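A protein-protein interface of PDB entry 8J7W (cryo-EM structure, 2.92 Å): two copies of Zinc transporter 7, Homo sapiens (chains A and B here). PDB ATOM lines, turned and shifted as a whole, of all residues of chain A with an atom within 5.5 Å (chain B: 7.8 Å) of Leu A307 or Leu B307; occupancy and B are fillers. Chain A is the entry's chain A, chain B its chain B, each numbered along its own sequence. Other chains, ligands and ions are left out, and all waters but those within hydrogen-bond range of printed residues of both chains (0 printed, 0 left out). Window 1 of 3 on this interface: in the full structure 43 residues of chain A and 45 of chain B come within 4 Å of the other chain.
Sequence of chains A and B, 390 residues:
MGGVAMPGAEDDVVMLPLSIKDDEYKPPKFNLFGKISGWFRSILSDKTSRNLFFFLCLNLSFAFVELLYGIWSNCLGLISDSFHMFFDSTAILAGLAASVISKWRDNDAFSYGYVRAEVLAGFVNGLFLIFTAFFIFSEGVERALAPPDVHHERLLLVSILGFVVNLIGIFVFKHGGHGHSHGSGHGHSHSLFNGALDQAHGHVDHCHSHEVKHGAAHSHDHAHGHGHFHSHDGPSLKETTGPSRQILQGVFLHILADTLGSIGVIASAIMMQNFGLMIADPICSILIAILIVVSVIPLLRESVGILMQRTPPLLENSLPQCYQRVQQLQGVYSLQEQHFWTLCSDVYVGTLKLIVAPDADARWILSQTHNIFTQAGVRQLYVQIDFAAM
The guanidinium group (NH2) of Arg A116 sits at hydrogen-bond distance from the backbone carbonyl oxygen (O) of Ile A306 (3.4 Å). NH2 of Arg B116 sits at hydrogen-bond distance from O of Thr B342 (3.0 Å). The guanidinium group (NH2) of Arg B116 sits at hydrogen-bond distance from the side-chain amide oxygen (OE1) of Gln B309. The guanidinium group of Arg A116 lies within hydrogen-bond range of the side-chain amide oxygen of Gln A309 (2.8 Å). The backbone carbonyl oxygen (O) of Leu B343 lies within hydrogen-bond range of the guanidinium group (NE) of Arg B116 (2.9 Å).
Arg B116 touches Arg A116. Phe B123 touches Leu A120. CD1 of Leu A120 touches CG of Met B308, 3.8 Å away. CE2 of Phe A123 touches CD2 of Leu B120 (3.9 Å). Phe A123 touches Phe B123 (CD2 to CE2, 3.8 Å). Phe A123 touches Val B124 (CZ to CG2, 3.5 Å). Leu B307 touches Leu A307 (CD2 to O, 3.7 Å). Phe B110 touches Met A308 (CE2 to CE, 3.6 Å). SD of Met A308 touches C of Arg B116, 3.8 Å away. CD1 of Leu B120 touches CG of Met A308 (3.6 Å).
Printed residues of chain B within 4 Å of Leu A120: Phe B123 and Met B308. Glu A302 touches none of the printed residues of chain B. Printed residues of chain A within 4 Å of Leu B120: Phe A123 and Met A308. Printed residues of chain A within 4 Å of Phe B123: Leu A120 and Phe A123. Glu B302 touches none of the printed residues of chain A. Of chain A, only Arg A116 and Leu A307 come within 4 Å of Leu B307. Of the printed residues of chain A, Gln B309 touches Arg A116 (3.0 Å) and Gln A309 (3.4 Å). The nearest residue of chain A that does not touch Leu B307 is Leu A120 (4.1 Å).
Of the 24 printed residues of chain B, 9 touch a printed residue of chain A. Hydrophobic or aromatic side chains of chain A that line the printed part of chain B: Leu A120, Phe A123 and Met A308. Among the printed residues, no Asp or Glu carboxylate lies within 4 Å of a Lys or Arg side-chain nitrogen of the other chain.
NH1 of Arg B116 sits at hydrogen-bond distance from O of Leu A307, 2.9 Å away. The side-chain amide oxygen of Gln B309 sits at hydrogen-bond distance from the guanidinium group of Arg A116 (3.0 Å). O of Leu B307 sits at hydrogen-bond distance from NH1 of Arg A116 (3.0 Å). The backbone NH (N) of Ala B117 sits at hydrogen-bond distance from the side-chain sulfur (SD) of Met A308 (3.6 Å). OE1 of Gln A309 lies close to OE1 of Gln B309 (3.4 Å). The guanidinium group (NH1) of Arg B116 sits at hydrogen-bond distance from the side-chain amide oxygen (OE1) of Gln A309 (3.3 Å).
Arg B116 touches its own counterpart, Arg A116. Arg A116 touches Gln B309, and with the chains exchanged Gln A309 touches Arg B116. Leu A120 touches Met B308, and with the chains exchanged Met A308 touches Leu B120. Leu B307 touches its own counterpart, Leu A307. Positions printed for both chains: 116, 119, 120, 123, 302, 303, 304, 305, 306, 307, 308 and 309. Of the 17 pairs that touch across the chains among the printed residues, 14 have their exchanged pair printed and touching as well.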
ATOM      1  N   ARG A 116      -3.392  27.477 -24.868  1.00  0.00           N
ATOM      2  CA  ARG A 116      -2.660  26.262 -25.196  1.00  0.00           C
ATOM      3  C   ARG A 116      -3.393  25.404 -26.217  1.00  0.00           C
ATOM      4  O   ARG A 116      -2.869  24.360 -26.623  1.00  0.00           O
ATOM      5  CB  ARG A 116      -2.387  25.452 -23.928  1.00  0.00           C
ATOM      6  CG  ARG A 116      -1.131  25.878 -23.191  1.00  0.00           C
ATOM      7  CD  ARG A 116      -0.024  24.859 -23.349  1.00  0.00           C
ATOM      8  NE  ARG A 116       1.227  25.318 -22.760  1.00  0.00           N
ATOM      9  CZ  ARG A 116       1.900  24.662 -21.826  1.00  0.00           C
ATOM     10  NH1 ARG A 116       1.467  23.509 -21.344  1.00  0.00           N
ATOM     11  NH2 ARG A 116       3.035  25.174 -21.365  1.00  0.00           N
ATOM     12  N   VAL A 119      -1.328  25.144 -29.405  1.00  0.00           N
ATOM     13  CA  VAL A 119      -0.236  24.185 -29.268  1.00  0.00           C
ATOM     14  C   VAL A 119      -0.767  22.761 -29.347  1.00  0.00           C
ATOM     15  O   VAL A 119      -0.186  21.900 -30.023  1.00  0.00           O
ATOM     16  CB  VAL A 119       0.527  24.432 -27.954  1.00  0.00           C
ATOM     17  CG1 VAL A 119       1.761  23.551 -27.885  1.00  0.00           C
ATOM     18  CG2 VAL A 119       0.896  25.900 -27.821  1.00  0.00           C
ATOM     19  N   LEU A 120      -1.883  22.494 -28.664  1.00  0.00           N
ATOM     20  CA  LEU A 120      -2.469  21.159 -28.704  1.00  0.00           C
ATOM     21  C   LEU A 120      -2.944  20.803 -30.107  1.00  0.00           C
ATOM     22  O   LEU A 120      -2.827  19.651 -30.532  1.00  0.00           O
ATOM     23  CB  LEU A 120      -3.616  21.061 -27.701  1.00  0.00           C
ATOM     24  CG  LEU A 120      -3.214  20.706 -26.269  1.00  0.00           C
ATOM     25  CD1 LEU A 120      -4.442  20.420 -25.424  1.00  0.00           C
ATOM     26  CD2 LEU A 120      -2.262  19.525 -26.253  1.00  0.00           C
ATOM     27  N   PHE A 123       0.023  19.868 -32.144  1.00  0.00           N
ATOM     28  CA  PHE A 123       0.473  18.541 -31.737  1.00  0.00           C
ATOM     29  C   PHE A 123      -0.395  17.445 -32.350  1.00  0.00           C
ATOM     30  O   PHE A 123       0.118  16.494 -32.959  1.00  0.00           O
ATOM     31  CB  PHE A 123       0.460  18.455 -30.212  1.00  0.00           C
ATOM     32  CG  PHE A 123       1.165  17.255 -29.666  1.00  0.00           C
ATOM     33  CD1 PHE A 123       2.464  16.973 -30.040  1.00  0.00           C
ATOM     34  CD2 PHE A 123       0.534  16.415 -28.769  1.00  0.00           C
ATOM     35  CE1 PHE A 123       3.117  15.874 -29.536  1.00  0.00           C
ATOM     36  CE2 PHE A 123       1.183  15.315 -28.260  1.00  0.00           C
ATOM     37  CZ  PHE A 123       2.477  15.045 -28.643  1.00  0.00           C
ATOM     38  N   GLU A 302       8.692  21.146 -31.668  1.00  0.00           N
ATOM     39  CA  GLU A 302       8.354  22.393 -30.984  1.00  0.00           C
ATOM     40  C   GLU A 302       7.159  22.210 -30.052  1.00  0.00           C
ATOM     41  O   GLU A 302       7.159  22.725 -28.925  1.00  0.00           O
ATOM     42  CB  GLU A 302       8.086  23.497 -32.008  1.00  0.00           C
ATOM     43  CG  GLU A 302       6.914  24.409 -31.680  1.00  0.00           C
ATOM     44  CD  GLU A 302       6.892  25.660 -32.534  1.00  0.00           C
ATOM     45  OE1 GLU A 302       7.387  25.605 -33.680  1.00  0.00           O
ATOM     46  OE2 GLU A 302       6.380  26.695 -32.060  1.00  0.00           O
ATOM     47  N   SER A 303       6.140  21.467 -30.495  1.00  0.00           N
ATOM     48  CA  SER A 303       4.969  21.234 -29.656  1.00  0.00           C
ATOM     49  C   SER A 303       5.326  20.422 -28.418  1.00  0.00           C
ATOM     50  O   SER A 303       4.847  20.716 -27.317  1.00  0.00           O
ATOM     51  CB  SER A 303       3.881  20.528 -30.463  1.00  0.00           C
ATOM     52  OG  SER A 303       3.724  21.129 -31.735  1.00  0.00           O
ATOM     53  N   VAL A 304       6.165  19.395 -28.579  1.00  0.00           N
ATOM     54  CA  VAL A 304       6.596  18.595 -27.439  1.00  0.00           C
ATOM     55  C   VAL A 304       7.408  19.444 -26.473  1.00  0.00           C
ATOM     56  O   VAL A 304       7.238  19.353 -25.253  1.00  0.00           O
ATOM     57  CB  VAL A 304       7.382  17.360 -27.924  1.00  0.00           C
ATOM     58  CG1 VAL A 304       8.356  16.875 -26.861  1.00  0.00           C
ATOM     59  CG2 VAL A 304       6.426  16.249 -28.306  1.00  0.00           C
ATOM     60  N   GLY A 305       8.288  20.297 -27.003  1.00  0.00           N
ATOM     61  CA  GLY A 305       9.041  21.193 -26.141  1.00  0.00           C
ATOM     62  C   GLY A 305       8.151  22.126 -25.342  1.00  0.00           C
ATOM     63  O   GLY A 305       8.391  22.361 -24.156  1.00  0.00           O
ATOM     64  N   ILE A 306       7.113  22.668 -25.977  1.00  0.00           N
ATOM     65  CA  ILE A 306       6.206  23.566 -25.266  1.00  0.00           C
ATOM     66  C   ILE A 306       5.425  22.805 -24.197  1.00  0.00           C
ATOM     67  O   ILE A 306       5.327  23.249 -23.046  1.00  0.00           O
ATOM     68  CB  ILE A 306       5.266  24.282 -26.252  1.00  0.00           C
ATOM     69  CG1 ILE A 306       6.055  25.260 -27.120  1.00  0.00           C
ATOM     70  CG2 ILE A 306       4.176  25.028 -25.503  1.00  0.00           C
ATOM     71  CD1 ILE A 306       5.195  26.055 -28.076  1.00  0.00           C
ATOM     72  N   LEU A 307       4.876  21.643 -24.550  1.00  0.00           N
ATOM     73  CA  LEU A 307       4.034  20.898 -23.621  1.00  0.00           C
ATOM     74  C   LEU A 307       4.814  20.159 -22.542  1.00  0.00           C
ATOM     75  O   LEU A 307       4.197  19.646 -21.603  1.00  0.00           O
ATOM     76  CB  LEU A 307       3.157  19.899 -24.380  1.00  0.00           C
ATOM     77  CG  LEU A 307       2.210  20.476 -25.431  1.00  0.00           C
ATOM     78  CD1 LEU A 307       1.690  19.376 -26.338  1.00  0.00           C
ATOM     79  CD2 LEU A 307       1.064  21.220 -24.767  1.00  0.00           C
ATOM     80  N   MET A 308       6.139  20.081 -22.641  1.00  0.00           N
ATOM     81  CA  MET A 308       6.954  19.452 -21.611  1.00  0.00           C
ATOM     82  C   MET A 308       7.507  20.458 -20.613  1.00  0.00           C
ATOM     83  O   MET A 308       8.371  20.100 -19.806  1.00  0.00           O
ATOM     84  CB  MET A 308       8.099  18.658 -22.240  1.00  0.00           C
ATOM     85  CG  MET A 308       7.671  17.326 -22.834  1.00  0.00           C
ATOM     86  SD  MET A 308       7.971  15.916 -21.759  1.00  0.00           S
ATOM     87  CE  MET A 308       9.723  16.083 -21.462  1.00  0.00           C
ATOM     88  N   GLN A 309       7.028  21.704 -20.656  1.00  0.00           N
ATOM     89  CA  GLN A 309       7.481  22.784 -19.777  1.00  0.00           C
ATOM     90  C   GLN A 309       8.980  23.034 -19.928  1.00  0.00           C
ATOM     91  O   GLN A 309       9.680  23.339 -18.962  1.00  0.00           O
ATOM     92  CB  GLN A 309       7.111  22.507 -18.318  1.00  0.00           C
ATOM     93  CG  GLN A 309       5.623  22.309 -18.091  1.00  0.00           C
ATOM     94  CD  GLN A 309       4.816  23.560 -18.368  1.00  0.00           C
ATOM     95  OE1 GLN A 309       4.002  23.596 -19.285  1.00  0.00           O
ATOM     96  NE2 GLN A 309       5.036  24.591 -17.570  1.00  0.00           N
ATOM     97  N   PHE B 110      15.342  21.650 -19.681  1.00  0.00           N
ATOM     98  CA  PHE B 110      14.156  21.109 -19.023  1.00  0.00           C
ATOM     99  C   PHE B 110      14.288  21.405 -17.534  1.00  0.00           C
ATOM    100  O   PHE B 110      14.796  20.592 -16.762  1.00  0.00           O
ATOM    101  CB  PHE B 110      14.006  19.620 -19.311  1.00  0.00           C
ATOM    102  CG  PHE B 110      13.574  19.321 -20.718  1.00  0.00           C
ATOM    103  CD1 PHE B 110      14.502  19.266 -21.745  1.00  0.00           C
ATOM    104  CD2 PHE B 110      12.239  19.120 -21.020  1.00  0.00           C
ATOM    105  CE1 PHE B 110      14.109  19.002 -23.040  1.00  0.00           C
ATOM    106  CE2 PHE B 110      11.839  18.856 -22.315  1.00  0.00           C
ATOM    107  CZ  PHE B 110      12.775  18.796 -23.324  1.00  0.00           C
ATOM    108  N   VAL B 115       9.061  15.123 -16.217  1.00  0.00           N
ATOM    109  CA  VAL B 115       7.888  14.565 -15.557  1.00  0.00           C
ATOM    110  C   VAL B 115       6.626  14.710 -16.395  1.00  0.00           C
ATOM    111  O   VAL B 115       5.621  14.050 -16.111  1.00  0.00           O
ATOM    112  CB  VAL B 115       7.707  15.222 -14.180  1.00  0.00           C
ATOM    113  CG1 VAL B 115       8.893  14.904 -13.289  1.00  0.00           C
ATOM    114  CG2 VAL B 115       7.550  16.719 -14.336  1.00  0.00           C
ATOM    115  N   ARG B 116       6.641  15.565 -17.418  1.00  0.00           N
ATOM    116  CA  ARG B 116       5.507  15.687 -18.323  1.00  0.00           C
ATOM    117  C   ARG B 116       5.445  14.548 -19.331  1.00  0.00           C
ATOM    118  O   ARG B 116       4.487  14.479 -20.111  1.00  0.00           O
ATOM    119  CB  ARG B 116       5.566  17.027 -19.061  1.00  0.00           C
ATOM    120  CG  ARG B 116       4.915  18.186 -18.322  1.00  0.00           C
ATOM    121  CD  ARG B 116       3.406  18.064 -18.303  1.00  0.00           C
ATOM    122  NE  ARG B 116       2.777  19.136 -17.540  1.00  0.00           N
ATOM    123  CZ  ARG B 116       2.440  20.319 -18.035  1.00  0.00           C
ATOM    124  NH1 ARG B 116       2.652  20.624 -19.303  1.00  0.00           N
ATOM    125  NH2 ARG B 116       1.871  21.217 -17.238  1.00  0.00           N
ATOM    126  N   ALA B 117       6.445  13.663 -19.328  1.00  0.00           N
ATOM    127  CA  ALA B 117       6.509  12.593 -20.317  1.00  0.00           C
ATOM    128  C   ALA B 117       5.378  11.588 -20.134  1.00  0.00           C
ATOM    129  O   ALA B 117       4.858  11.060 -21.119  1.00  0.00           O
ATOM    130  CB  ALA B 117       7.864  11.893 -20.248  1.00  0.00           C
ATOM    131  N   VAL B 119       2.319  12.221 -18.920  1.00  0.00           N
ATOM    132  CA  VAL B 119       1.114  12.869 -19.424  1.00  0.00           C
ATOM    133  C   VAL B 119       1.115  12.874 -20.945  1.00  0.00           C
ATOM    134  O   VAL B 119       0.100  12.567 -21.583  1.00  0.00           O
ATOM    135  CB  VAL B 119       0.995  14.294 -18.855  1.00  0.00           C
ATOM    136  CG1 VAL B 119      -0.387  14.862 -19.131  1.00  0.00           C
ATOM    137  CG2 VAL B 119       1.294  14.301 -17.365  1.00  0.00           C
ATOM    138  N   LEU B 120       2.260  13.203 -21.548  1.00  0.00           N
ATOM    139  CA  LEU B 120       2.340  13.235 -23.004  1.00  0.00           C
ATOM    140  C   LEU B 120       2.172  11.846 -23.606  1.00  0.00           C
ATOM    141  O   LEU B 120       1.547  11.697 -24.657  1.00  0.00           O
ATOM    142  CB  LEU B 120       3.661  13.858 -23.451  1.00  0.00           C
ATOM    143  CG  LEU B 120       3.606  15.352 -23.777  1.00  0.00           C
ATOM    144  CD1 LEU B 120       4.858  15.781 -24.511  1.00  0.00           C
ATOM    145  CD2 LEU B 120       2.371  15.681 -24.595  1.00  0.00           C
ATOM    146  N   ALA B 121       2.720  10.817 -22.958  1.00  0.00           N
ATOM    147  CA  ALA B 121       2.588   9.458 -23.474  1.00  0.00           C
ATOM    148  C   ALA B 121       1.143   8.983 -23.413  1.00  0.00           C
ATOM    149  O   ALA B 121       0.632   8.395 -24.378  1.00  0.00           O
ATOM    150  CB  ALA B 121       3.497   8.511 -22.694  1.00  0.00           C
ATOM    151  N   GLY B 122       0.467   9.229 -22.287  1.00  0.00           N
ATOM    152  CA  GLY B 122      -0.946   8.893 -22.202  1.00  0.00           C
ATOM    153  C   GLY B 122      -1.774   9.633 -23.236  1.00  0.00           C
ATOM    154  O   GLY B 122      -2.642   9.047 -23.891  1.00  0.00           O
ATOM    155  N   PHE B 123      -1.495  10.927 -23.411  1.00  0.00           N
ATOM    156  CA  PHE B 123      -2.206  11.723 -24.406  1.00  0.00           C
ATOM    157  C   PHE B 123      -1.977  11.190 -25.814  1.00  0.00           C
ATOM    158  O   PHE B 123      -2.926  11.059 -26.598  1.00  0.00           O
ATOM    159  CB  PHE B 123      -1.757  13.180 -24.300  1.00  0.00           C
ATOM    160  CG  PHE B 123      -2.557  14.127 -25.138  1.00  0.00           C
ATOM    161  CD1 PHE B 123      -3.921  14.255 -24.952  1.00  0.00           C
ATOM    162  CD2 PHE B 123      -1.942  14.905 -26.102  1.00  0.00           C
ATOM    163  CE1 PHE B 123      -4.657  15.131 -25.718  1.00  0.00           C
ATOM    164  CE2 PHE B 123      -2.673  15.784 -26.869  1.00  0.00           C
ATOM    165  CZ  PHE B 123      -4.033  15.897 -26.677  1.00  0.00           C
ATOM    166  N   VAL B 124      -0.727  10.861 -26.148  1.00  0.00           N
ATOM    167  CA  VAL B 124      -0.397  10.392 -27.488  1.00  0.00           C
ATOM    168  C   VAL B 124      -1.062   9.054 -27.767  1.00  0.00           C
ATOM    169  O   VAL B 124      -1.598   8.831 -28.859  1.00  0.00           O
ATOM    170  CB  VAL B 124       1.131  10.316 -27.663  1.00  0.00           C
ATOM    171  CG1 VAL B 124       1.501   9.439 -28.846  1.00  0.00           C
ATOM    172  CG2 VAL B 124       1.703  11.703 -27.851  1.00  0.00           C
ATOM    173  N   LEU B 127      -4.747   9.587 -28.345  1.00  0.00           N
ATOM    174  CA  LEU B 127      -4.959  10.127 -29.684  1.00  0.00           C
ATOM    175  C   LEU B 127      -4.808   9.047 -30.747  1.00  0.00           C
ATOM    176  O   LEU B 127      -5.573   9.008 -31.717  1.00  0.00           O
ATOM    177  CB  LEU B 127      -3.979  11.264 -29.953  1.00  0.00           C
ATOM    178  CG  LEU B 127      -4.151  12.545 -29.148  1.00  0.00           C
ATOM    179  CD1 LEU B 127      -3.036  13.496 -29.501  1.00  0.00           C
ATOM    180  CD2 LEU B 127      -5.504  13.171 -29.421  1.00  0.00           C
ATOM    181  N   LEU B 300      -8.166  11.210 -22.152  1.00  0.00           N
ATOM    182  CA  LEU B 300      -7.932  12.387 -22.978  1.00  0.00           C
ATOM    183  C   LEU B 300      -8.358  13.657 -22.258  1.00  0.00           C
ATOM    184  O   LEU B 300      -7.686  14.688 -22.362  1.00  0.00           O
ATOM    185  CB  LEU B 300      -8.672  12.256 -24.309  1.00  0.00           C
ATOM    186  CG  LEU B 300      -7.974  11.465 -25.414  1.00  0.00           C
ATOM    187  CD1 LEU B 300      -8.617  11.755 -26.756  1.00  0.00           C
ATOM    188  CD2 LEU B 300      -6.489  11.771 -25.453  1.00  0.00           C
ATOM    189  N   ARG B 301      -9.473  13.605 -21.528  1.00  0.00           N
ATOM    190  CA  ARG B 301      -9.926  14.771 -20.776  1.00  0.00           C
ATOM    191  C   ARG B 301      -8.912  15.162 -19.709  1.00  0.00           C
ATOM    192  O   ARG B 301      -8.574  16.342 -19.558  1.00  0.00           O
ATOM    193  CB  ARG B 301     -11.287  14.487 -20.141  1.00  0.00           C
ATOM    194  CG  ARG B 301     -12.467  14.686 -21.075  1.00  0.00           C
ATOM    195  CD  ARG B 301     -13.764  14.902 -20.307  1.00  0.00           C
ATOM    196  NE  ARG B 301     -13.656  14.500 -18.909  1.00  0.00           N
ATOM    197  CZ  ARG B 301     -13.856  15.311 -17.880  1.00  0.00           C
ATOM    198  NH1 ARG B 301     -14.178  16.582 -18.054  1.00  0.00           N
ATOM    199  NH2 ARG B 301     -13.731  14.835 -16.645  1.00  0.00           N
ATOM    200  N   GLU B 302      -8.402  14.173 -18.970  1.00  0.00           N
ATOM    201  CA  GLU B 302      -7.413  14.462 -17.932  1.00  0.00           C
ATOM    202  C   GLU B 302      -6.120  15.012 -18.527  1.00  0.00           C
ATOM    203  O   GLU B 302      -5.548  15.982 -18.010  1.00  0.00           O
ATOM    204  CB  GLU B 302      -7.135  13.203 -17.113  1.00  0.00           C
ATOM    205  CG  GLU B 302      -6.745  13.474 -15.671  1.00  0.00           C
ATOM    206  CD  GLU B 302      -5.637  12.563 -15.186  1.00  0.00           C
ATOM    207  OE1 GLU B 302      -5.469  11.469 -15.765  1.00  0.00           O
ATOM    208  OE2 GLU B 302      -4.934  12.939 -14.225  1.00  0.00           O
ATOM    209  N   SER B 303      -5.651  14.409 -19.624  1.00  0.00           N
ATOM    210  CA  SER B 303      -4.419  14.867 -20.261  1.00  0.00           C
ATOM    211  C   SER B 303      -4.576  16.268 -20.837  1.00  0.00           C
ATOM    212  O   SER B 303      -3.657  17.090 -20.739  1.00  0.00           O
ATOM    213  CB  SER B 303      -4.000  13.883 -21.349  1.00  0.00           C
ATOM    214  OG  SER B 303      -4.126  12.548 -20.899  1.00  0.00           O
ATOM    215  N   VAL B 304      -5.725  16.556 -21.450  1.00  0.00           N
ATOM    216  CA  VAL B 304      -5.978  17.888 -21.987  1.00  0.00           C
ATOM    217  C   VAL B 304      -6.029  18.910 -20.862  1.00  0.00           C
ATOM    218  O   VAL B 304      -5.474  20.006 -20.981  1.00  0.00           O
ATOM    219  CB  VAL B 304      -7.272  17.885 -22.823  1.00  0.00           C
ATOM    220  CG1 VAL B 304      -7.860  19.283 -22.926  1.00  0.00           C
ATOM    221  CG2 VAL B 304      -7.003  17.329 -24.204  1.00  0.00           C
ATOM    222  N   GLY B 305      -6.677  18.564 -19.749  1.00  0.00           N
ATOM    223  CA  GLY B 305      -6.709  19.471 -18.616  1.00  0.00           C
ATOM    224  C   GLY B 305      -5.326  19.781 -18.074  1.00  0.00           C
ATOM    225  O   GLY B 305      -5.015  20.933 -17.772  1.00  0.00           O
ATOM    226  N   ILE B 306      -4.479  18.759 -17.948  1.00  0.00           N
ATOM    227  CA  ILE B 306      -3.128  18.992 -17.441  1.00  0.00           C
ATOM    228  C   ILE B 306      -2.321  19.833 -18.426  1.00  0.00           C
ATOM    229  O   ILE B 306      -1.673  20.814 -18.041  1.00  0.00           O
ATOM    230  CB  ILE B 306      -2.431  17.657 -17.127  1.00  0.00           C
ATOM    231  CG1 ILE B 306      -3.010  17.052 -15.848  1.00  0.00           C
ATOM    232  CG2 ILE B 306      -0.933  17.860 -16.979  1.00  0.00           C
ATOM    233  CD1 ILE B 306      -2.294  15.810 -15.380  1.00  0.00           C
ATOM    234  N   LEU B 307      -2.362  19.479 -19.711  1.00  0.00           N
ATOM    235  CA  LEU B 307      -1.544  20.157 -20.711  1.00  0.00           C
ATOM    236  C   LEU B 307      -2.045  21.549 -21.069  1.00  0.00           C
ATOM    237  O   LEU B 307      -1.290  22.318 -21.674  1.00  0.00           O
ATOM    238  CB  LEU B 307      -1.452  19.312 -21.983  1.00  0.00           C
ATOM    239  CG  LEU B 307      -0.679  17.997 -21.877  1.00  0.00           C
ATOM    240  CD1 LEU B 307      -0.783  17.215 -23.175  1.00  0.00           C
ATOM    241  CD2 LEU B 307       0.774  18.250 -21.516  1.00  0.00           C
ATOM    242  N   MET B 308      -3.280  21.900 -20.719  1.00  0.00           N
ATOM    243  CA  MET B 308      -3.819  23.222 -21.010  1.00  0.00           C
ATOM    244  C   MET B 308      -3.553  24.219 -19.892  1.00  0.00           C
ATOM    245  O   MET B 308      -4.115  25.318 -19.918  1.00  0.00           O
ATOM    246  CB  MET B 308      -5.324  23.139 -21.279  1.00  0.00           C
ATOM    247  CG  MET B 308      -5.682  22.764 -22.708  1.00  0.00           C
ATOM    248  SD  MET B 308      -5.890  24.189 -23.789  1.00  0.00           S
ATOM    249  CE  MET B 308      -7.608  24.581 -23.504  1.00  0.00           C
ATOM    250  N   GLN B 309      -2.712  23.854 -18.921  1.00  0.00           N
ATOM    251  CA  GLN B 309      -2.402  24.686 -17.757  1.00  0.00           C
ATOM    252  C   GLN B 309      -3.662  25.027 -16.966  1.00  0.00           C
ATOM    253  O   GLN B 309      -3.815  26.134 -16.448  1.00  0.00           O
ATOM    254  CB  GLN B 309      -1.644  25.954 -18.159  1.00  0.00           C
ATOM    255  CG  GLN B 309      -0.361  25.691 -18.924  1.00  0.00           C
ATOM    256  CD  GLN B 309       0.605  24.810 -18.161  1.00  0.00           C
ATOM    257  OE1 GLN B 309       0.715  23.618 -18.428  1.00  0.00           O
ATOM    258  NE2 GLN B 309       1.310  25.395 -17.207  1.00  0.00           N
ATOM    259  N   ARG B 310      -4.570  24.064 -16.875  1.00  0.00           N
ATOM    260  CA  ARG B 310      -5.778  24.223 -16.083  1.00  0.00           C
ATOM    261  C   ARG B 310      -5.454  24.065 -14.602  1.00  0.00           C
ATOM    262  O   ARG B 310      -4.554  23.311 -14.219  1.00  0.00           O
ATOM    263  CB  ARG B 310      -6.832  23.200 -16.516  1.00  0.00           C
ATOM    264  CG  ARG B 310      -8.057  23.114 -15.630  1.00  0.00           C
ATOM    265  CD  ARG B 310      -8.849  21.842 -15.857  1.00  0.00           C
ATOM    266  NE  ARG B 310     -10.259  21.998 -15.516  1.00  0.00           N
ATOM    267  CZ  ARG B 310     -10.729  22.190 -14.290  1.00  0.00           C
ATOM    268  NH1 ARG B 310      -9.933  22.215 -13.234  1.00  0.00           N
ATOM    269  NH2 ARG B 310     -12.039  22.348 -14.117  1.00  0.00           N
ATOM    270  N   THR B 342      -0.988  21.921 -12.908  1.00  0.00           N
ATOM    271  CA  THR B 342      -0.483  20.596 -12.582  1.00  0.00           C
ATOM    272  C   THR B 342       0.770  20.325 -13.404  1.00  0.00           C
ATOM    273  O   THR B 342       0.720  20.329 -14.638  1.00  0.00           O
ATOM    274  CB  THR B 342      -1.545  19.533 -12.866  1.00  0.00           C
ATOM    275  OG1 THR B 342      -2.839  20.052 -12.542  1.00  0.00           O
ATOM    276  CG2 THR B 342      -1.294  18.299 -12.038  1.00  0.00           C
ATOM    277  N   LEU B 343       1.890  20.091 -12.721  1.00  0.00           N
ATOM    278  CA  LEU B 343       3.116  19.710 -13.412  1.00  0.00           C
ATOM    279  C   LEU B 343       3.077  18.237 -13.796  1.00  0.00           C
ATOM    280  O   LEU B 343       3.129  17.885 -14.979  1.00  0.00           O
ATOM    281  CB  LEU B 343       4.329  20.006 -12.528  1.00  0.00           C
ATOM    282  CG  LEU B 343       5.695  19.613 -13.086  1.00  0.00           C
ATOM    283  CD1 LEU B 343       5.977  20.346 -14.388  1.00  0.00           C
ATOM    284  CD2 LEU B 343       6.785  19.882 -12.066  1.00  0.00           C
